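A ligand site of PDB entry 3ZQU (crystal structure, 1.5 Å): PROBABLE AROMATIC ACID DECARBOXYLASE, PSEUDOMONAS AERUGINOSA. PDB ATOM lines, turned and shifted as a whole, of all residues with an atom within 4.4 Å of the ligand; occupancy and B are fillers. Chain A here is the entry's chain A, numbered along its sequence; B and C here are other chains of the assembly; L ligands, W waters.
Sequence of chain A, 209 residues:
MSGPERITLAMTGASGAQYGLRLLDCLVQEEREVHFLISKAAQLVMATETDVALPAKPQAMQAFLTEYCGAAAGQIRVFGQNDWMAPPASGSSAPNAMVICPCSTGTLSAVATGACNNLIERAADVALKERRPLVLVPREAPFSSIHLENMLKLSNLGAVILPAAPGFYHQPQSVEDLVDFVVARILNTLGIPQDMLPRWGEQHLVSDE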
ATOM      1  N   THR A  12     -31.077  12.094   8.762  1.00  0.00           N
ATOM      2  CA  THR A  12     -30.510  12.649   7.555  1.00  0.00           C
ATOM      3  C   THR A  12     -29.161  13.336   7.886  1.00  0.00           C
ATOM      4  O   THR A  12     -28.767  13.405   9.078  1.00  0.00           O
ATOM      5  CB  THR A  12     -31.494  13.620   6.848  1.00  0.00           C
ATOM      6  OG1 THR A  12     -31.734  14.732   7.739  1.00  0.00           O
ATOM      7  CG2 THR A  12     -32.812  12.949   6.531  1.00  0.00           C
ATOM      8  N   GLY A  13     -28.460  13.806   6.851  1.00  0.00           N
ATOM      9  CA  GLY A  13     -27.027  14.086   6.933  1.00  0.00           C
ATOM     10  C   GLY A  13     -26.611  15.400   7.600  1.00  0.00           C
ATOM     11  O   GLY A  13     -25.672  16.009   7.173  1.00  0.00           O
ATOM     12  N   ALA A  14     -27.332  15.843   8.621  1.00  0.00           N
ATOM     13  CA  ALA A  14     -26.764  16.896   9.481  1.00  0.00           C
ATOM     14  C   ALA A  14     -25.883  16.278  10.560  1.00  0.00           C
ATOM     15  O   ALA A  14     -26.114  15.111  10.967  1.00  0.00           O
ATOM     16  CB  ALA A  14     -27.860  17.715  10.137  1.00  0.00           C
ATOM     17  N   SER A  15     -24.927  17.052  11.080  1.00  0.00           N
ATOM     18  CA  SER A  15     -24.204  16.666  12.277  1.00  0.00           C
ATOM     19  C   SER A  15     -25.164  16.427  13.433  1.00  0.00           C
ATOM     20  O   SER A  15     -26.227  17.071  13.555  1.00  0.00           O
ATOM     21  CB  SER A  15     -23.163  17.730  12.602  1.00  0.00           C
ATOM     22  OG  SER A  15     -22.282  17.222  13.589  1.00  0.00           O
ATOM     23  N   SER A  39     -30.591   8.350   5.457  1.00  0.00           N
ATOM     24  CA  SER A  39     -30.084   8.748   4.184  1.00  0.00           C
ATOM     25  C   SER A  39     -28.637   8.315   3.957  1.00  0.00           C
ATOM     26  O   SER A  39     -27.905   8.004   4.911  1.00  0.00           O
ATOM     27  CB  SER A  39     -30.197  10.295   4.022  1.00  0.00           C
ATOM     28  OG  SER A  39     -29.167  10.945   4.745  1.00  0.00           O
ATOM     29  N   ALA A  41     -26.151  10.296   3.066  1.00  0.00           N
ATOM     30  CA  ALA A  41     -25.253  11.227   3.722  1.00  0.00           C
ATOM     31  C   ALA A  41     -25.259  10.965   5.233  1.00  0.00           C
ATOM     32  O   ALA A  41     -24.233  11.107   5.894  1.00  0.00           O
ATOM     33  CB  ALA A  41     -25.714  12.685   3.415  1.00  0.00           C
ATOM     34  N   ALA A  42     -26.415  10.634   5.827  1.00  0.00           N
ATOM     35  CA  ALA A  42     -26.447  10.332   7.251  1.00  0.00           C
ATOM     36  C   ALA A  42     -25.606   9.106   7.636  1.00  0.00           C
ATOM     37  O   ALA A  42     -25.063   9.093   8.727  1.00  0.00           O
ATOM     38  CB  ALA A  42     -27.854  10.161   7.819  1.00  0.00           C
ATOM     39  N   VAL A  45     -22.238  10.572   8.004  1.00  0.00           N
ATOM     40  CA  VAL A  45     -22.108  11.321   9.226  1.00  0.00           C
ATOM     41  C   VAL A  45     -21.940  10.341  10.425  1.00  0.00           C
ATOM     42  O   VAL A  45     -21.076  10.560  11.297  1.00  0.00           O
ATOM     43  CB  VAL A  45     -23.386  12.198   9.509  1.00  0.00           C
ATOM     44  CG1 VAL A  45     -23.269  12.865  10.890  1.00  0.00           C
ATOM     45  CG2 VAL A  45     -23.505  13.297   8.437  1.00  0.00           C
ATOM     46  N   THR A  48     -18.441   9.047  10.550  1.00  0.00           N
ATOM     47  CA  THR A  48     -17.501  10.143  10.888  1.00  0.00           C
ATOM     48  C   THR A  48     -17.552  10.512  12.364  1.00  0.00           C
ATOM     49  O   THR A  48     -16.502  10.723  12.958  1.00  0.00           O
ATOM     50  CB  THR A  48     -17.908  11.429  10.079  1.00  0.00           C
ATOM     51  OG1 THR A  48     -17.949  11.132   8.689  1.00  0.00           O
ATOM     52  CG2 THR A  48     -16.899  12.578  10.259  1.00  0.00           C
ATOM     53  N   SER A 104     -31.120  17.571   8.043  1.00  0.00           N
ATOM     54  CA  SER A 104     -30.230  18.416   7.249  1.00  0.00           C
ATOM     55  C   SER A 104     -31.038  19.579   6.616  1.00  0.00           C
ATOM     56  O   SER A 104     -32.286  19.520   6.476  1.00  0.00           O
ATOM     57  CB  SER A 104     -29.612  17.585   6.119  1.00  0.00           C
ATOM     58  OG  SER A 104     -30.615  17.206   5.163  1.00  0.00           O
ATOM     59  N   THR A 105     -30.291  20.601   6.191  1.00  0.00           N
ATOM     60  CA  THR A 105     -30.997  21.733   5.544  1.00  0.00           C
ATOM     61  C   THR A 105     -31.581  21.246   4.208  1.00  0.00           C
ATOM     62  O   THR A 105     -32.643  21.749   3.776  1.00  0.00           O
ATOM     63  CB  THR A 105     -30.119  22.981   5.365  1.00  0.00           C
ATOM     64  OG1 THR A 105     -29.045  22.650   4.518  1.00  0.00           O
ATOM     65  CG2 THR A 105     -29.609  23.470   6.728  1.00  0.00           C
ATOM     66  N   GLY A 106     -30.921  20.268   3.538  1.00  0.00           N
ATOM     67  CA  GLY A 106     -31.433  19.728   2.299  1.00  0.00           C
ATOM     68  C   GLY A 106     -32.758  18.996   2.496  1.00  0.00           C
ATOM     69  O   GLY A 106     -33.646  19.111   1.623  1.00  0.00           O
ATOM     70  N   THR A 107     -32.880  18.196   3.562  1.00  0.00           N
ATOM     71  CA  THR A 107     -34.127  17.521   3.824  1.00  0.00           C
ATOM     72  C   THR A 107     -35.217  18.492   4.253  1.00  0.00           C
ATOM     73  O   THR A 107     -36.366  18.396   3.802  1.00  0.00           O
ATOM     74  CB  THR A 107     -33.964  16.371   4.777  1.00  0.00           C
ATOM     75  OG1 THR A 107     -33.248  15.333   4.068  1.00  0.00           O
ATOM     76  CG2 THR A 107     -35.327  15.813   5.234  1.00  0.00           C
ATOM     77  N   ARG A 139     -29.952  20.814  12.507  1.00  0.00           N
ATOM     78  CA  ARG A 139     -28.687  21.165  13.175  1.00  0.00           C
ATOM     79  C   ARG A 139     -27.851  21.906  12.140  1.00  0.00           C
ATOM     80  O   ARG A 139     -27.426  21.293  11.151  1.00  0.00           O
ATOM     81  CB  ARG A 139     -27.900  19.881  13.570  1.00  0.00           C
ATOM     82  CG  ARG A 139     -26.841  20.044  14.720  1.00  0.00           C
ATOM     83  CD  ARG A 139     -25.854  21.238  14.550  1.00  0.00           C
ATOM     84  NE  ARG A 139     -25.099  21.183  13.317  1.00  0.00           N
ATOM     85  CZ  ARG A 139     -24.255  22.170  12.929  1.00  0.00           C
ATOM     86  NH1 ARG A 139     -24.028  23.247  13.679  1.00  0.00           N
ATOM     87  NH2 ARG A 139     -23.631  22.048  11.774  1.00  0.00           N
ATOM     88  N   GLU A 140     -27.729  23.227  12.295  1.00  0.00           N
ATOM     89  CA  GLU A 140     -26.999  24.033  11.321  1.00  0.00           C
ATOM     90  C   GLU A 140     -26.726  25.321  12.064  1.00  0.00           C
ATOM     91  O   GLU A 140     -27.452  25.704  12.992  1.00  0.00           O
ATOM     92  CB  GLU A 140     -27.894  24.286  10.076  1.00  0.00           C
ATOM     93  CG  GLU A 140     -27.207  25.224   9.008  1.00  0.00           C
ATOM     94  CD  GLU A 140     -25.921  24.643   8.514  1.00  0.00           C
ATOM     95  OE1 GLU A 140     -24.884  24.874   9.203  1.00  0.00           O
ATOM     96  OE2 GLU A 140     -25.942  23.938   7.494  1.00  0.00           O
ATOM     97  N   TRP B  84     -18.560  15.382   0.679  1.00  0.00           N
ATOM     98  CA  TRP B  84     -18.923  16.262   1.819  1.00  0.00           C
ATOM     99  C   TRP B  84     -17.751  16.576   2.732  1.00  0.00           C
ATOM    100  O   TRP B  84     -17.870  17.355   3.657  1.00  0.00           O
ATOM    101  CB  TRP B  84     -20.056  15.619   2.629  1.00  0.00           C
ATOM    102  CG  TRP B  84     -21.191  15.164   1.778  1.00  0.00           C
ATOM    103  CD1 TRP B  84     -21.603  13.890   1.612  1.00  0.00           C
ATOM    104  CD2 TRP B  84     -22.048  15.978   0.945  1.00  0.00           C
ATOM    105  NE1 TRP B  84     -22.659  13.836   0.725  1.00  0.00           N
ATOM    106  CE2 TRP B  84     -22.947  15.111   0.309  1.00  0.00           C
ATOM    107  CE3 TRP B  84     -22.127  17.358   0.681  1.00  0.00           C
ATOM    108  CZ2 TRP B  84     -23.923  15.547  -0.608  1.00  0.00           C
ATOM    109  CZ3 TRP B  84     -23.119  17.810  -0.224  1.00  0.00           C
ATOM    110  CH2 TRP B  84     -24.008  16.911  -0.847  1.00  0.00           C
ATOM    111  N   CYS B 116     -29.615  21.458  -1.681  1.00  0.00           N
ATOM    112  CA  CYS B 116     -28.352  20.771  -1.224  1.00  0.00           C
ATOM    113  C   CYS B 116     -28.246  19.298  -1.699  1.00  0.00           C
ATOM    114  O   CYS B 116     -27.800  18.447  -0.938  1.00  0.00           O
ATOM    115  CB  CYS B 116     -28.259  20.802   0.308  1.00  0.00           C
ATOM    116  SG  CYS B 116     -28.043  22.390   1.023  1.00  0.00           S
ATOM    117  N   ARG B 122     -24.960  22.363  -2.120  1.00  0.00           N
ATOM    118  CA  ARG B 122     -24.607  22.592  -0.724  1.00  0.00           C
ATOM    119  C   ARG B 122     -23.594  23.731  -0.622  1.00  0.00           C
ATOM    120  O   ARG B 122     -23.679  24.511   0.321  1.00  0.00           O
ATOM    121  CB  ARG B 122     -24.000  21.307  -0.099  1.00  0.00           C
ATOM    122  CG  ARG B 122     -23.529  21.478   1.342  1.00  0.00           C
ATOM    123  CD  ARG B 122     -24.586  21.990   2.349  1.00  0.00           C
ATOM    124  NE  ARG B 122     -23.997  22.005   3.710  1.00  0.00           N
ATOM    125  CZ  ARG B 122     -24.605  22.523   4.758  1.00  0.00           C
ATOM    126  NH1 ARG B 122     -25.820  23.118   4.652  1.00  0.00           N
ATOM    127  NH2 ARG B 122     -23.967  22.494   5.937  1.00  0.00           N
ATOM    128  N   TYR C 169     -19.042  17.035  14.507  1.00  0.00           N
ATOM    129  CA  TYR C 169     -18.204  16.398  13.489  1.00  0.00           C
ATOM    130  C   TYR C 169     -16.733  16.423  13.834  1.00  0.00           C
ATOM    131  O   TYR C 169     -15.937  15.862  13.069  1.00  0.00           O
ATOM    132  CB  TYR C 169     -18.443  16.926  12.081  1.00  0.00           C
ATOM    133  CG  TYR C 169     -18.571  18.425  11.911  1.00  0.00           C
ATOM    134  CD1 TYR C 169     -17.448  19.247  11.942  1.00  0.00           C
ATOM    135  CD2 TYR C 169     -19.812  19.006  11.673  1.00  0.00           C
ATOM    136  CE1 TYR C 169     -17.525  20.623  11.721  1.00  0.00           C
ATOM    137  CE2 TYR C 169     -19.932  20.386  11.467  1.00  0.00           C
ATOM    138  CZ  TYR C 169     -18.802  21.176  11.480  1.00  0.00           C
ATOM    139  OH  TYR C 169     -18.892  22.526  11.251  1.00  0.00           O
ATOM    140  N   TRP C 200     -12.600  23.186   7.880  1.00  0.00           N
ATOM    141  CA  TRP C 200     -13.050  21.951   7.228  1.00  0.00           C
ATOM    142  C   TRP C 200     -12.387  21.714   5.876  1.00  0.00           C
ATOM    143  O   TRP C 200     -12.416  22.557   4.966  1.00  0.00           O
ATOM    144  CB  TRP C 200     -14.570  22.022   6.978  1.00  0.00           C
ATOM    145  CG  TRP C 200     -15.180  20.769   6.507  1.00  0.00           C
ATOM    146  CD1 TRP C 200     -15.635  20.461   5.216  1.00  0.00           C
ATOM    147  CD2 TRP C 200     -15.535  19.653   7.325  1.00  0.00           C
ATOM    148  NE1 TRP C 200     -16.188  19.203   5.205  1.00  0.00           N
ATOM    149  CE2 TRP C 200     -16.163  18.691   6.485  1.00  0.00           C
ATOM    150  CE3 TRP C 200     -15.369  19.355   8.699  1.00  0.00           C
ATOM    151  CZ2 TRP C 200     -16.615  17.447   6.956  1.00  0.00           C
ATOM    152  CZ3 TRP C 200     -15.839  18.104   9.182  1.00  0.00           C
ATOM    153  CH2 TRP C 200     -16.480  17.174   8.299  1.00  0.00           C
HETATM  154  C1  LIG L   1     -22.852  17.293   6.560  1.00  0.00           C
HETATM  155  N1  LIG L   1     -23.870  18.136   6.012  1.00  0.00           N
HETATM  156  C2  LIG L   1     -24.556  18.892   6.939  1.00  0.00           C
HETATM  157  N2  LIG L   1     -25.781  19.404   6.466  1.00  0.00           N
HETATM  158  C3  LIG L   1     -26.516  20.178   7.374  1.00  0.00           C
HETATM  159  O1  LIG L   1     -27.616  20.632   7.006  1.00  0.00           O
HETATM  160  N3  LIG L   1     -26.165  20.366   8.690  1.00  0.00           N
HETATM  161  C4  LIG L   1     -24.926  19.831   9.179  1.00  0.00           C
HETATM  162  O2  LIG L   1     -24.647  19.919  10.372  1.00  0.00           O
HETATM  163  C5  LIG L   1     -24.151  19.098   8.262  1.00  0.00           C
HETATM  164  N4  LIG L   1     -22.938  18.518   8.677  1.00  0.00           N
HETATM  165  C6  LIG L   1     -22.423  17.501   7.878  1.00  0.00           C
HETATM  166  C7  LIG L   1     -21.396  16.734   8.427  1.00  0.00           C
HETATM  167  C8  LIG L   1     -20.884  15.682   7.669  1.00  0.00           C
HETATM  168  C9  LIG L   1     -19.752  14.831   8.322  1.00  0.00           C
HETATM  169  C10 LIG L   1     -21.304  15.438   6.377  1.00  0.00           C
HETATM  170  C11 LIG L   1     -20.719  14.262   5.576  1.00  0.00           C
HETATM  171  C12 LIG L   1     -22.322  16.231   5.806  1.00  0.00           C
HETATM  172  C13 LIG L   1     -24.218  18.183   4.539  1.00  0.00           C
HETATM  173  C14 LIG L   1     -25.357  17.243   4.153  1.00  0.00           C
HETATM  174  O3  LIG L   1     -25.054  15.868   4.538  1.00  0.00           O
HETATM  175  C15 LIG L   1     -25.591  17.333   2.631  1.00  0.00           C
HETATM  176  O4  LIG L   1     -26.096  18.670   2.337  1.00  0.00           O
HETATM  177  C16 LIG L   1     -26.568  16.248   2.176  1.00  0.00           C
HETATM  178  O5  LIG L   1     -26.881  16.559   0.831  1.00  0.00           O
HETATM  179  C17 LIG L   1     -27.822  16.061   3.033  1.00  0.00           C
HETATM  180  O6  LIG L   1     -28.559  14.991   2.429  1.00  0.00           O
HETATM  181  P1  LIG L   1     -29.651  14.262   3.162  1.00  0.00           P
HETATM  182  O7  LIG L   1     -30.346  13.350   2.052  1.00  0.00           O
HETATM  183  O8  LIG L   1     -30.689  15.372   3.585  1.00  0.00           O
HETATM  184  O9  LIG L   1     -29.121  13.505   4.288  1.00  0.00           O
HETATM  185  O   HOH W   1     -27.837  20.006   4.063  1.00  0.00           O
HETATM  186  O   HOH W   2     -21.810  20.726   6.515  1.00  0.00           O
HETATM  187  O   HOH W   3     -29.772  21.138   9.644  1.00  0.00           O
HETATM  188  O   HOH W   4     -27.612  14.792  -1.027  1.00  0.00           O
HETATM  189  O   HOH W   5     -32.579  15.758   1.003  1.00  0.00           O
HETATM  190  O   HOH W   6     -28.271  11.473   1.320  1.00  0.00           O
HETATM  191  O   HOH W   7     -30.141  17.103   0.646  1.00  0.00           O
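The side-chain hydroxyl (OG) of Ser 104 sits at hydrogen-bond distance from an oxygen (O8) of the ligand (2.4 Å). An oxygen (O9) of the ligand sits at hydrogen-bond distance from the side-chain hydroxyl (OG) of Ser 39. The side-chain hydroxyl (OG1) of Thr 107 lies within hydrogen-bond range of an oxygen (O8) of the ligand (2.6 Å). N of Gly 13 sits at hydrogen-bond distance from O9 of the ligand (2.7 Å). O of Gly 13 lies within hydrogen-bond range of O3 of the ligand (2.7 Å). O of Arg 139 lies within hydrogen-bond range of N3 of the ligand. The guanidinium group of Arg 139 lies within hydrogen-bond range of an oxygen (O2) of the ligand, 2.7 Å away. An oxygen (O5) of the ligand sits at hydrogen-bond distance from the backbone carbonyl oxygen (O) of Cys 116 of chain B, 2.7 Å away. N of Thr 105 lies within hydrogen-bond range of O1 of the ligand (2.8 Å). An oxygen (O2) of the ligand is in hydrogen-bond range of the backbone NH of Ser 15 (3.0 Å).
The side-chain hydroxyl (OG) of Ser 104 is in hydrogen-bond range of the backbone NH (N) of Thr 107, at 2.9 Å. N of Ser 104 is in hydrogen-bond range of OG1 of Thr 12, at 2.9 Å. N of Gly 106 sits close to OG of Ser 104, 3.5 Å away. OG of Ser 39 is in hydrogen-bond range of N of Ala 42 (3.0 Å). The side-chain sulfur of Cys 116 of chain B sits at hydrogen-bond distance from the side-chain hydroxyl of Thr 105 (3.6 Å). The side-chain hydroxyl (OG1) of Thr 105 sits at hydrogen-bond distance from the guanidinium group (NH1) of Arg 122 of chain B (3.3 Å). The backbone carbonyl oxygen of Trp 84 of chain B is in hydrogen-bond range of the indole nitrogen of Trp 200 of chain C. NH2 of Arg 122 of chain B is in salt-bridge range of OE2 of Glu 140 (2.9 Å).
Thr 12 touches the ligand (CB to O9, 3.5 Å). Ala 14 touches the ligand (CB to N3, 3.5 Å). CB of Ala 41 touches O3 of the ligand (3.4 Å). Val 45 touches the ligand. OE2 of Glu 140 touches O1 of the ligand, at 3.7 Å. Trp 84 of chain B touches the ligand (CB to C11, 3.3 Å). Arg 122 of chain B touches the ligand. Within 4 Å of the ligand: Thr 12, Gly 13, Ala 14, Ser 15, Ser 39, Ala 41, Val 45, Ser 104, Thr 105, Thr 107, Arg 139, Glu 140, Trp 84 of chain B, Cys 116 of chain B and Arg 122 of chain B. Along chain A the residues within 4 Å of the ligand span positions 12 to 140.
Water W1 lies within hydrogen-bond range of an oxygen (O4) of the ligand (2.8 Å), the side-chain hydroxyl (OG1) of Thr 105 (2.9 Å) and the backbone NH (N) of Gly 106 (3.1 Å). Water W6 bridges an oxygen (O7) of the ligand (2.9 Å) and the backbone NH (N) of Ala 41 (3.0 Å). Water W7 bridges the backbone carbonyl oxygen (O) of Cys 116 of chain B (3.1 Å) and an oxygen (O6) of the ligand (3.2 Å). Water W5 lies within hydrogen-bond range of the side-chain hydroxyl (OG1) of Thr 107 (3.2 Å) and an oxygen (O8) of the ligand (3.2 Å). Water W2 bridges the guanidinium group (NH2) of Arg 122 of chain B (2.8 Å) and a nitrogen (N4) of the ligand (3.3 Å). Water W3 lies within hydrogen-bond range of O of Arg 139 (2.8 Å) and O1 of the ligand (3.4 Å).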
